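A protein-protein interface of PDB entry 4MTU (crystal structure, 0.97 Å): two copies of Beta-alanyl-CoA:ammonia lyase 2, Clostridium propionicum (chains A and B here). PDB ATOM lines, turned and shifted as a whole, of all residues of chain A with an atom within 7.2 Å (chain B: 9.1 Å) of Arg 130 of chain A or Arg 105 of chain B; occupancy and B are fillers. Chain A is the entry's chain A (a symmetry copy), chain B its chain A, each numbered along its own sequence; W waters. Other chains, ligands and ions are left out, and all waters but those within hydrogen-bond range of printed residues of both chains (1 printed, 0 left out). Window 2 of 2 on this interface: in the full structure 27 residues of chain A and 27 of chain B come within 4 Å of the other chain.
The side-chain hydroxyl (OG1) of Thr 104 of chain B sits at hydrogen-bond distance from the side-chain carboxylate (OD2) of Asp 47 of chain A, at 2.6 Å. The backbone NH (N) of Ile 48 of chain A is in hydrogen-bond range of the backbone carbonyl oxygen (O) of Thr 104 of chain B, 3.1 Å away. O of Gly 46 of chain A sits at hydrogen-bond distance from N of Ala 106 of chain B. NH2 of Arg 130 of chain A is in hydrogen-bond range of O of Ala 106 of chain B (2.8 Å). OG1 of Thr 107 of chain B is in hydrogen-bond range of OE1 of Gln 133 of chain A.
The backbone NH of Thr 107 of chain B lies within hydrogen-bond range of the backbone carbonyl oxygen of Lys 94 of chain B. N of Val 96 of chain B is in hydrogen-bond range of O of Arg 105 of chain B (2.9 Å). The guanidinium group of Arg 105 of chain B is in salt-bridge range of the side-chain carboxylate of Asp 103 of chain B (2.8 Å). O of Asp 47 of chain A sits at hydrogen-bond distance from N of Val 42 of chain A (3.4 Å). O of Asp 45 of chain A is in hydrogen-bond range of N of Arg 130 of chain A, 2.9 Å away. The side-chain amide nitrogen (NE2) of Gln 133 of chain A sits at hydrogen-bond distance from the backbone carbonyl oxygen (O) of Gly 131 of chain A.
Val 42 of chain A touches Ala 106 of chain B. Val 42 of chain A touches Thr 107 of chain B. Gly 46 of chain A touches Arg 105 of chain B. Ile 48 of chain A touches Met 95 of chain B (CG2 to SD, 3.7 Å). Val 96 of chain B touches Arg 130 of chain A. Arg 105 of chain B touches Arg 130 of chain A (CG to NE, 3.6 Å). Gln 133 of chain A touches Ala 106 of chain B (CG to O, 3.99 Å). Ala 108 of chain B touches Gln 133 of chain A (CB to O, 3.4 Å).
Arg 130 of chain A touches just these residues of chain B: Val 96, Arg 105 and Ala 106. Arg 105 of chain B touches two residues of chain A. Gly 46 of chain A touches just these residues of chain B: Arg 105 (3.4 Å) and Ala 106 (3.0 Å). No residue of chain B comes within 4 Å of Gly 131 of chain A. Of the printed residues of chain A, Thr 107 of chain B touches Val 42 (3.5 Å) and Gln 133 (2.7 Å). Of the printed residues of chain A, Thr 104 of chain B touches Asp 47 (2.6 Å) and Ile 48 (3.1 Å). Of the printed residues of chain B, Val 42 of chain A touches Ala 106 (3.7 Å) and Thr 107 (3.5 Å). Of the printed residues of chain B, Asp 47 of chain A touches Thr 104 (2.6 Å). Of the printed residues of chain A, Met 95 of chain B touches Ile 48 (3.7 Å). Asn 100 of chain B touches none of the printed residues of chain A. Val 65 of chain B touches none of the printed residues of chain A. The nearest residue of chain B that does not touch Arg 130 of chain A is Thr 107 of chain B (4.2 Å). The nearest residue of chain A that does not touch Arg 105 of chain B is Asp 47 of chain A (4.1 Å).
Of the 18 printed residues of chain B, 7 touch a printed residue of chain A. Hydrophobic or aromatic side chains of chain B within 4 Å of the printed part of chain A: Met 95, Val 96, Ala 106 and Ala 108. Along chain B the printed residues that touch a printed residue of chain A span positions 95 to 108. Of the 17 printed residues of chain A, 6 touch a printed residue of chain B. Printed residues of chain A that touch a printed residue of chain B: Val 42, Gly 46, Asp 47, Ile 48, Arg 130 and Gln 133. Hydrophobic or aromatic side chains of chain A within 4 Å of the printed part of chain B: Val 42 and Ile 48. Among the printed residues, 13 pairs touch across the chains. Among the printed residues, no Asp or Glu carboxylate lies within 4 Å of a Lys or Arg side-chain nitrogen of the other chain.
No position is printed for both chains. Of the 13 pairs that touch across the chains among the printed residues, none has its exchanged pair printed and touching as well.
Water W1 lies within hydrogen-bond range of the guanidinium group of Arg 105 of chain B and the guanidinium group of Arg 130 of chain A.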
ATOM      1  N   VAL A  42       9.950 -19.405 -31.055  1.00  0.00           N
ATOM      2  CA  VAL A  42      10.478 -19.980 -29.827  1.00  0.00           C
ATOM      3  C   VAL A  42      11.988 -19.774 -29.770  1.00  0.00           C
ATOM      4  O   VAL A  42      12.559 -19.380 -28.743  1.00  0.00           O
ATOM      5  CB  VAL A  42      10.099 -21.492 -29.720  1.00  0.00           C
ATOM      6  CG1 VAL A  42      10.831 -22.132 -28.529  1.00  0.00           C
ATOM      7  CG2 VAL A  42       8.578 -21.639 -29.603  1.00  0.00           C
ATOM      8  N   VAL A  44      13.957 -17.605 -31.509  1.00  0.00           N
ATOM      9  CA  VAL A  44      14.492 -16.237 -31.588  1.00  0.00           C
ATOM     10  C   VAL A  44      14.187 -15.431 -30.336  1.00  0.00           C
ATOM     11  O   VAL A  44      14.966 -14.536 -29.973  1.00  0.00           O
ATOM     12  CB  VAL A  44      14.015 -15.508 -32.877  1.00  0.00           C
ATOM     13  CG1 VAL A  44      12.613 -15.023 -32.778  1.00  0.00           C
ATOM     14  CG2 VAL A  44      15.024 -14.401 -33.194  1.00  0.00           C
ATOM     15  N   ASP A  45      13.057 -15.690 -29.669  1.00  0.00           N
ATOM     16  CA  ASP A  45      12.645 -14.842 -28.533  1.00  0.00           C
ATOM     17  C   ASP A  45      11.836 -15.575 -27.473  1.00  0.00           C
ATOM     18  O   ASP A  45      11.299 -14.900 -26.574  1.00  0.00           O
ATOM     19  CB  ASP A  45      12.034 -13.541 -28.971  1.00  0.00           C
ATOM     20  CG  ASP A  45      12.976 -12.375 -29.091  1.00  0.00           C
ATOM     21  OD1 ASP A  45      12.981 -11.643 -30.094  1.00  0.00           O
ATOM     22  OD2 ASP A  45      13.813 -12.172 -28.150  1.00  0.00           O
ATOM     23  N   GLY A  46      11.757 -16.890 -27.490  1.00  0.00           N
ATOM     24  CA  GLY A  46      11.250 -17.604 -26.347  1.00  0.00           C
ATOM     25  C   GLY A  46       9.757 -17.494 -26.083  1.00  0.00           C
ATOM     26  O   GLY A  46       9.330 -17.646 -24.923  1.00  0.00           O
ATOM     27  N   ASP A  47       8.965 -17.308 -27.132  1.00  0.00           N
ATOM     28  CA  ASP A  47       7.513 -17.196 -27.019  1.00  0.00           C
ATOM     29  C   ASP A  47       6.891 -17.861 -28.254  1.00  0.00           C
ATOM     30  O   ASP A  47       7.493 -17.777 -29.331  1.00  0.00           O
ATOM     31  CB  ASP A  47       7.114 -15.737 -26.925  1.00  0.00           C
ATOM     32  CG  ASP A  47       5.677 -15.544 -26.499  1.00  0.00           C
ATOM     33  OD1 ASP A  47       4.768 -15.534 -27.386  1.00  0.00           O
ATOM     34  OD2 ASP A  47       5.409 -15.410 -25.279  1.00  0.00           O
ATOM     35  N   ILE A  48       5.742 -18.448 -28.100  1.00  0.00           N
ATOM     36  CA  ILE A  48       5.112 -19.106 -29.259  1.00  0.00           C
ATOM     37  C   ILE A  48       4.613 -18.100 -30.293  1.00  0.00           C
ATOM     38  O   ILE A  48       4.442 -18.507 -31.451  1.00  0.00           O
ATOM     39  CB  ILE A  48       3.982 -20.055 -28.865  1.00  0.00           C
ATOM     40  CG1 ILE A  48       2.851 -19.366 -28.054  1.00  0.00           C
ATOM     41  CG2 ILE A  48       4.564 -21.265 -28.154  1.00  0.00           C
ATOM     42  CD1 ILE A  48       1.585 -20.218 -27.943  1.00  0.00           C
ATOM     43  N   TYR A  83       8.373 -10.136 -37.049  1.00  0.00           N
ATOM     44  CA  TYR A  83       9.415 -10.953 -37.606  1.00  0.00           C
ATOM     45  C   TYR A  83       8.955 -11.434 -38.996  1.00  0.00           C
ATOM     46  O   TYR A  83       7.882 -12.042 -39.100  1.00  0.00           O
ATOM     47  CB  TYR A  83       9.698 -12.160 -36.704  1.00  0.00           C
ATOM     48  CG  TYR A  83       9.982 -11.840 -35.275  1.00  0.00           C
ATOM     49  CD1 TYR A  83       8.990 -11.492 -34.388  1.00  0.00           C
ATOM     50  CD2 TYR A  83      11.284 -11.914 -34.775  1.00  0.00           C
ATOM     51  CE1 TYR A  83       9.220 -11.192 -33.068  1.00  0.00           C
ATOM     52  CE2 TYR A  83      11.514 -11.595 -33.423  1.00  0.00           C
ATOM     53  CZ  TYR A  83      10.508 -11.256 -32.582  1.00  0.00           C
ATOM     54  OH  TYR A  83      10.723 -10.960 -31.255  1.00  0.00           O
ATOM     55  N   ILE A 124       5.670 -10.882 -31.557  1.00  0.00           N
ATOM     56  CA  ILE A 124       5.824 -11.125 -30.118  1.00  0.00           C
ATOM     57  C   ILE A 124       5.821  -9.740 -29.456  1.00  0.00           C
ATOM     58  O   ILE A 124       6.690  -8.928 -29.755  1.00  0.00           O
ATOM     59  CB  ILE A 124       7.065 -11.898 -29.723  1.00  0.00           C
ATOM     60  CG1 ILE A 124       7.204 -13.208 -30.468  1.00  0.00           C
ATOM     61  CG2 ILE A 124       7.103 -12.086 -28.192  1.00  0.00           C
ATOM     62  CD1 ILE A 124       8.565 -13.864 -30.330  1.00  0.00           C
ATOM     63  N   ALA A 125       4.879  -9.476 -28.556  1.00  0.00           N
ATOM     64  CA  ALA A 125       4.838  -8.172 -27.858  1.00  0.00           C
ATOM     65  C   ALA A 125       6.170  -7.987 -27.111  1.00  0.00           C
ATOM     66  O   ALA A 125       6.755  -8.938 -26.600  1.00  0.00           O
ATOM     67  CB  ALA A 125       3.693  -8.122 -26.880  1.00  0.00           C
ATOM     68  N   LYS A 126       6.619  -6.774 -27.067  1.00  0.00           N
ATOM     69  CA  LYS A 126       7.916  -6.464 -26.480  1.00  0.00           C
ATOM     70  C   LYS A 126       8.073  -7.048 -25.095  1.00  0.00           C
ATOM     71  O   LYS A 126       9.155  -7.623 -24.790  1.00  0.00           O
ATOM     72  CB  LYS A 126       8.142  -4.942 -26.552  1.00  0.00           C
ATOM     73  CG  LYS A 126       9.598  -4.640 -26.806  1.00  0.00           C
ATOM     74  CD  LYS A 126      10.135  -5.037 -28.227  1.00  0.00           C
ATOM     75  CE  LYS A 126      11.661  -5.131 -28.091  1.00  0.00           C
ATOM     76  NZ  LYS A 126      12.390  -5.432 -29.362  1.00  0.00           N
ATOM     77  N   ASP A 127       7.042  -6.963 -24.276  1.00  0.00           N
ATOM     78  CA  ASP A 127       7.130  -7.433 -22.886  1.00  0.00           C
ATOM     79  C   ASP A 127       7.280  -8.963 -22.809  1.00  0.00           C
ATOM     80  O   ASP A 127       7.664  -9.488 -21.771  1.00  0.00           O
ATOM     81  CB  ASP A 127       5.941  -7.000 -22.034  1.00  0.00           C
ATOM     82  CG  ASP A 127       5.773  -5.527 -21.761  1.00  0.00           C
ATOM     83  OD1 ASP A 127       6.749  -4.749 -21.995  1.00  0.00           O
ATOM     84  OD2 ASP A 127       4.697  -5.020 -21.353  1.00  0.00           O
ATOM     85  N   ASN A 128       6.880  -9.706 -23.858  1.00  0.00           N
ATOM     86  CA  ASN A 128       6.947 -11.129 -23.913  1.00  0.00           C
ATOM     87  C   ASN A 128       8.205 -11.650 -24.605  1.00  0.00           C
ATOM     88  O   ASN A 128       8.410 -12.890 -24.638  1.00  0.00           O
ATOM     89  CB  ASN A 128       5.751 -11.738 -24.649  1.00  0.00           C
ATOM     90  CG  ASN A 128       4.463 -11.531 -23.869  1.00  0.00           C
ATOM     91  OD1 ASN A 128       4.457 -11.597 -22.654  1.00  0.00           O
ATOM     92  ND2 ASN A 128       3.424 -11.190 -24.600  1.00  0.00           N
ATOM     93  N   GLN A 129       9.058 -10.796 -25.148  1.00  0.00           N
ATOM     94  CA  GLN A 129      10.297 -11.253 -25.775  1.00  0.00           C
ATOM     95  C   GLN A 129      11.325 -11.600 -24.672  1.00  0.00           C
ATOM     96  O   GLN A 129      11.501 -10.881 -23.693  1.00  0.00           O
ATOM     97  CB  GLN A 129      10.869 -10.205 -26.684  1.00  0.00           C
ATOM     98  CG  GLN A 129       9.968  -9.919 -27.896  1.00  0.00           C
ATOM     99  CD  GLN A 129      10.400  -8.766 -28.758  1.00  0.00           C
ATOM    100  OE1 GLN A 129      11.579  -8.344 -28.722  1.00  0.00           O
ATOM    101  NE2 GLN A 129       9.546  -8.269 -29.620  1.00  0.00           N
ATOM    102  N   ARG A 130      11.989 -12.735 -24.847  1.00  0.00           N
ATOM    103  CA  ARG A 130      12.899 -13.280 -23.830  1.00  0.00           C
ATOM    104  C   ARG A 130      14.299 -13.468 -24.310  1.00  0.00           C
ATOM    105  O   ARG A 130      15.144 -13.987 -23.584  1.00  0.00           O
ATOM    106  CB  ARG A 130      12.336 -14.567 -23.201  1.00  0.00           C
ATOM    107  CG  ARG A 130      10.934 -14.376 -22.647  1.00  0.00           C
ATOM    108  CD  ARG A 130      10.453 -15.477 -21.746  1.00  0.00           C
ATOM    109  NE  ARG A 130      10.593 -16.797 -22.411  1.00  0.00           N
ATOM    110  CZ  ARG A 130      11.299 -17.801 -22.000  1.00  0.00           C
ATOM    111  NH1 ARG A 130      11.950 -17.841 -20.845  1.00  0.00           N
ATOM    112  NH2 ARG A 130      11.362 -18.926 -22.743  1.00  0.00           N
ATOM    113  N   GLY A 131      14.597 -13.061 -25.543  1.00  0.00           N
ATOM    114  CA  GLY A 131      15.890 -13.259 -26.141  1.00  0.00           C
ATOM    115  C   GLY A 131      16.027 -14.704 -26.731  1.00  0.00           C
ATOM    116  O   GLY A 131      15.169 -15.571 -26.565  1.00  0.00           O
ATOM    117  N   PRO A 132      17.107 -14.899 -27.431  1.00  0.00           N
ATOM    118  CA  PRO A 132      17.316 -16.180 -28.138  1.00  0.00           C
ATOM    119  C   PRO A 132      17.337 -17.352 -27.165  1.00  0.00           C
ATOM    120  O   PRO A 132      17.850 -17.277 -26.055  1.00  0.00           O
ATOM    121  CB  PRO A 132      18.618 -16.013 -28.869  1.00  0.00           C
ATOM    122  CG  PRO A 132      18.838 -14.561 -29.002  1.00  0.00           C
ATOM    123  CD  PRO A 132      18.177 -13.945 -27.780  1.00  0.00           C
ATOM    124  N   GLN A 133      16.791 -18.501 -27.650  1.00  0.00           N
ATOM    125  CA  GLN A 133      16.691 -19.693 -26.886  1.00  0.00           C
ATOM    126  C   GLN A 133      17.492 -20.864 -27.425  1.00  0.00           C
ATOM    127  O   GLN A 133      17.571 -21.921 -26.813  1.00  0.00           O
ATOM    128  CB  GLN A 133      15.223 -20.161 -26.734  1.00  0.00           C
ATOM    129  CG  GLN A 133      14.338 -19.082 -26.123  1.00  0.00           C
ATOM    130  CD  GLN A 133      14.660 -18.769 -24.679  1.00  0.00           C
ATOM    131  OE1 GLN A 133      14.817 -19.674 -23.859  1.00  0.00           O
ATOM    132  NE2 GLN A 133      14.766 -17.479 -24.402  1.00  0.00           N
ATOM    133  N   VAL B  65       1.554 -31.165 -25.247  1.00  0.00           N
ATOM    134  CA  VAL B  65       1.160 -30.110 -26.199  1.00  0.00           C
ATOM    135  C   VAL B  65       2.246 -29.047 -26.176  1.00  0.00           C
ATOM    136  O   VAL B  65       2.716 -28.613 -25.106  1.00  0.00           O
ATOM    137  CB  VAL B  65      -0.194 -29.526 -25.802  1.00  0.00           C
ATOM    138  CG1 VAL B  65      -0.552 -28.339 -26.679  1.00  0.00           C
ATOM    139  CG2 VAL B  65      -1.269 -30.598 -25.877  1.00  0.00           C
ATOM    140  N   GLY B  66       2.636 -28.584 -27.379  1.00  0.00           N
ATOM    141  CA  GLY B  66       3.619 -27.550 -27.556  1.00  0.00           C
ATOM    142  C   GLY B  66       5.035 -28.044 -27.642  1.00  0.00           C
ATOM    143  O   GLY B  66       5.972 -27.283 -27.892  1.00  0.00           O
ATOM    144  N   ALA B  93      12.032 -28.773 -28.528  1.00  0.00           N
ATOM    145  CA  ALA B  93      11.538 -27.493 -27.980  1.00  0.00           C
ATOM    146  C   ALA B  93      10.283 -27.832 -27.186  1.00  0.00           C
ATOM    147  O   ALA B  93       9.682 -28.904 -27.401  1.00  0.00           O
ATOM    148  CB  ALA B  93      11.288 -26.469 -29.043  1.00  0.00           C
ATOM    149  N   LYS B  94       9.855 -26.912 -26.338  1.00  0.00           N
ATOM    150  CA  LYS B  94       8.729 -27.222 -25.428  1.00  0.00           C
ATOM    151  C   LYS B  94       8.210 -25.902 -24.827  1.00  0.00           C
ATOM    152  O   LYS B  94       8.941 -24.876 -24.793  1.00  0.00           O
ATOM    153  CB  LYS B  94       9.129 -28.143 -24.299  1.00  0.00           C
ATOM    154  CG  LYS B  94      10.259 -27.576 -23.449  1.00  0.00           C
ATOM    155  CD  LYS B  94      10.729 -28.447 -22.323  1.00  0.00           C
ATOM    156  CE  LYS B  94      11.559 -27.668 -21.291  1.00  0.00           C
ATOM    157  N   MET B  95       7.001 -25.917 -24.300  1.00  0.00           N
ATOM    158  CA  MET B  95       6.519 -24.851 -23.459  1.00  0.00           C
ATOM    159  C   MET B  95       7.281 -24.838 -22.129  1.00  0.00           C
ATOM    160  O   MET B  95       7.634 -25.898 -21.611  1.00  0.00           O
ATOM    161  CB  MET B  95       5.028 -25.028 -23.115  1.00  0.00           C
ATOM    162  CG  MET B  95       4.107 -25.131 -24.333  1.00  0.00           C
ATOM    163  SD  MET B  95       4.146 -23.749 -25.483  1.00  0.00           S
ATOM    164  CE  MET B  95       3.579 -22.375 -24.503  1.00  0.00           C
ATOM    165  N   VAL B  96       7.489 -23.669 -21.561  1.00  0.00           N
ATOM    166  CA  VAL B  96       8.156 -23.573 -20.226  1.00  0.00           C
ATOM    167  C   VAL B  96       7.256 -24.129 -19.117  1.00  0.00           C
ATOM    168  O   VAL B  96       7.789 -24.808 -18.235  1.00  0.00           O
ATOM    169  CB  VAL B  96       8.568 -22.143 -19.960  1.00  0.00           C
ATOM    170  CG1 VAL B  96       9.120 -21.996 -18.543  1.00  0.00           C
ATOM    171  CG2 VAL B  96       9.693 -21.737 -20.945  1.00  0.00           C
ATOM    172  N   ASP B  97       5.959 -23.823 -19.112  1.00  0.00           N
ATOM    173  CA  ASP B  97       5.070 -24.221 -18.024  1.00  0.00           C
ATOM    174  C   ASP B  97       3.733 -24.677 -18.553  1.00  0.00           C
ATOM    175  O   ASP B  97       2.769 -23.880 -18.697  1.00  0.00           O
ATOM    176  CB  ASP B  97       4.857 -23.089 -17.001  1.00  0.00           C
ATOM    177  CG  ASP B  97       4.017 -23.533 -15.820  1.00  0.00           C
ATOM    178  OD1 ASP B  97       3.661 -24.751 -15.733  1.00  0.00           O
ATOM    179  OD2 ASP B  97       3.679 -22.704 -14.980  1.00  0.00           O
ATOM    180  N   ILE B  98       3.599 -25.990 -18.817  1.00  0.00           N
ATOM    181  CA  ILE B  98       2.383 -26.558 -19.343  1.00  0.00           C
ATOM    182  C   ILE B  98       1.227 -26.405 -18.397  1.00  0.00           C
ATOM    183  O   ILE B  98       0.047 -26.534 -18.804  1.00  0.00           O
ATOM    184  CB  ILE B  98       2.606 -28.037 -19.768  1.00  0.00           C
ATOM    185  CG1 ILE B  98       1.570 -28.528 -20.770  1.00  0.00           C
ATOM    186  CG2 ILE B  98       2.585 -28.972 -18.559  1.00  0.00           C
ATOM    187  CD1 ILE B  98       1.620 -27.819 -22.105  1.00  0.00           C
ATOM    188  N   THR B  99       1.501 -26.238 -17.105  1.00  0.00           N
ATOM    189  CA  THR B  99       0.445 -26.160 -16.126  1.00  0.00           C
ATOM    190  C   THR B  99      -0.246 -24.807 -16.113  1.00  0.00           C
ATOM    191  O   THR B  99      -1.280 -24.676 -15.428  1.00  0.00           O
ATOM    192  CB  THR B  99       0.916 -26.448 -14.690  1.00  0.00           C
ATOM    193  OG1 THR B  99       1.644 -25.342 -14.138  1.00  0.00           O
ATOM    194  CG2 THR B  99       1.755 -27.741 -14.648  1.00  0.00           C
ATOM    195  N   ASN B 100       0.259 -23.806 -16.805  1.00  0.00           N
ATOM    196  CA  ASN B 100      -0.385 -22.492 -16.881  1.00  0.00           C
ATOM    197  C   ASN B 100      -0.814 -22.229 -18.309  1.00  0.00           C
ATOM    198  O   ASN B 100       0.016 -21.882 -19.139  1.00  0.00           O
ATOM    199  CB  ASN B 100       0.577 -21.395 -16.421  1.00  0.00           C
ATOM    200  CG  ASN B 100      -0.059 -20.037 -16.479  1.00  0.00           C
ATOM    201  OD1 ASN B 100      -1.198 -19.853 -16.957  1.00  0.00           O
ATOM    202  ND2 ASN B 100       0.692 -19.032 -16.000  1.00  0.00           N
ATOM    203  N   PRO B 101      -2.079 -22.467 -18.650  1.00  0.00           N
ATOM    204  CA  PRO B 101      -2.495 -22.346 -20.028  1.00  0.00           C
ATOM    205  C   PRO B 101      -2.291 -20.999 -20.659  1.00  0.00           C
ATOM    206  O   PRO B 101      -2.243 -20.940 -21.894  1.00  0.00           O
ATOM    207  CB  PRO B 101      -3.985 -22.700 -19.999  1.00  0.00           C
ATOM    208  CG  PRO B 101      -4.073 -23.596 -18.827  1.00  0.00           C
ATOM    209  CD  PRO B 101      -3.177 -22.973 -17.770  1.00  0.00           C
ATOM    210  N   GLN B 102      -2.208 -19.926 -19.904  1.00  0.00           N
ATOM    211  CA  GLN B 102      -1.992 -18.592 -20.421  1.00  0.00           C
ATOM    212  C   GLN B 102      -0.509 -18.272 -20.578  1.00  0.00           C
ATOM    213  O   GLN B 102      -0.220 -17.181 -21.098  1.00  0.00           O
ATOM    214  CB  GLN B 102      -2.759 -17.549 -19.615  1.00  0.00           C
ATOM    215  CG  GLN B 102      -4.257 -17.552 -19.941  1.00  0.00           C
ATOM    216  CD  GLN B 102      -5.037 -18.786 -19.582  1.00  0.00           C
ATOM    217  OE1 GLN B 102      -5.066 -19.191 -18.416  1.00  0.00           O
ATOM    218  NE2 GLN B 102      -5.655 -19.386 -20.570  1.00  0.00           N
ATOM    219  N   ASP B 103       0.378 -19.113 -20.135  1.00  0.00           N
ATOM    220  CA  ASP B 103       1.844 -18.847 -20.278  1.00  0.00           C
ATOM    221  C   ASP B 103       2.251 -19.203 -21.677  1.00  0.00           C
ATOM    222  O   ASP B 103       2.091 -20.372 -22.084  1.00  0.00           O
ATOM    223  CB  ASP B 103       2.595 -19.642 -19.226  1.00  0.00           C
ATOM    224  CG  ASP B 103       4.041 -19.268 -19.027  1.00  0.00           C
ATOM    225  OD1 ASP B 103       4.617 -18.606 -19.919  1.00  0.00           O
ATOM    226  OD2 ASP B 103       4.601 -19.652 -17.955  1.00  0.00           O
ATOM    227  N   THR B 104       2.735 -18.255 -22.441  1.00  0.00           N
ATOM    228  CA  THR B 104       3.147 -18.452 -23.828  1.00  0.00           C
ATOM    229  C   THR B 104       4.663 -18.661 -23.966  1.00  0.00           C
ATOM    230  O   THR B 104       5.155 -18.791 -25.096  1.00  0.00           O
ATOM    231  CB  THR B 104       2.672 -17.300 -24.712  1.00  0.00           C
ATOM    232  OG1 THR B 104       3.157 -16.048 -24.163  1.00  0.00           O
ATOM    233  CG2 THR B 104       1.152 -17.264 -24.853  1.00  0.00           C
ATOM    234  N   ARG B 105       5.396 -18.706 -22.850  1.00  0.00           N
ATOM    235  CA  ARG B 105       6.830 -18.894 -22.921  1.00  0.00           C
ATOM    236  C   ARG B 105       7.176 -20.289 -23.393  1.00  0.00           C
ATOM    237  O   ARG B 105       6.562 -21.278 -22.972  1.00  0.00           O
ATOM    238  CB  ARG B 105       7.471 -18.662 -21.546  1.00  0.00           C
ATOM    239  CG  ARG B 105       7.313 -17.272 -21.005  1.00  0.00           C
ATOM    240  CD  ARG B 105       7.959 -17.116 -19.622  1.00  0.00           C
ATOM    241  NE  ARG B 105       7.298 -17.994 -18.669  1.00  0.00           N
ATOM    242  CZ  ARG B 105       7.865 -18.566 -17.597  1.00  0.00           C
ATOM    243  NH1 ARG B 105       9.147 -18.379 -17.289  1.00  0.00           N
ATOM    244  NH2 ARG B 105       7.159 -19.388 -16.833  1.00  0.00           N
ATOM    245  N   ALA B 106       8.221 -20.381 -24.212  1.00  0.00           N
ATOM    246  CA  ALA B 106       8.680 -21.668 -24.733  1.00  0.00           C
ATOM    247  C   ALA B 106      10.175 -21.570 -24.964  1.00  0.00           C
ATOM    248  O   ALA B 106      10.741 -20.455 -25.064  1.00  0.00           O
ATOM    249  CB  ALA B 106       7.928 -22.043 -26.022  1.00  0.00           C
ATOM    250  N   THR B 107      10.861 -22.697 -25.028  1.00  0.00           N
ATOM    251  CA  THR B 107      12.289 -22.727 -25.178  1.00  0.00           C
ATOM    252  C   THR B 107      12.710 -23.958 -25.969  1.00  0.00           C
ATOM    253  O   THR B 107      11.940 -24.850 -26.223  1.00  0.00           O
ATOM    254  CB  THR B 107      12.979 -22.636 -23.814  1.00  0.00           C
ATOM    255  OG1 THR B 107      14.371 -22.353 -24.011  1.00  0.00           O
ATOM    256  CG2 THR B 107      12.827 -23.886 -23.010  1.00  0.00           C
ATOM    257  N   ALA B 108      13.982 -23.965 -26.364  1.00  0.00           N
ATOM    258  CA  ALA B 108      14.590 -25.088 -26.995  1.00  0.00           C
ATOM    259  C   ALA B 108      15.003 -26.111 -25.993  1.00  0.00           C
ATOM    260  O   ALA B 108      15.217 -25.788 -24.811  1.00  0.00           O
ATOM    261  CB  ALA B 108      15.773 -24.634 -27.842  1.00  0.00           C
HETATM  262  O   HOH W   1      11.161 -16.611 -18.218  1.00  0.00           O
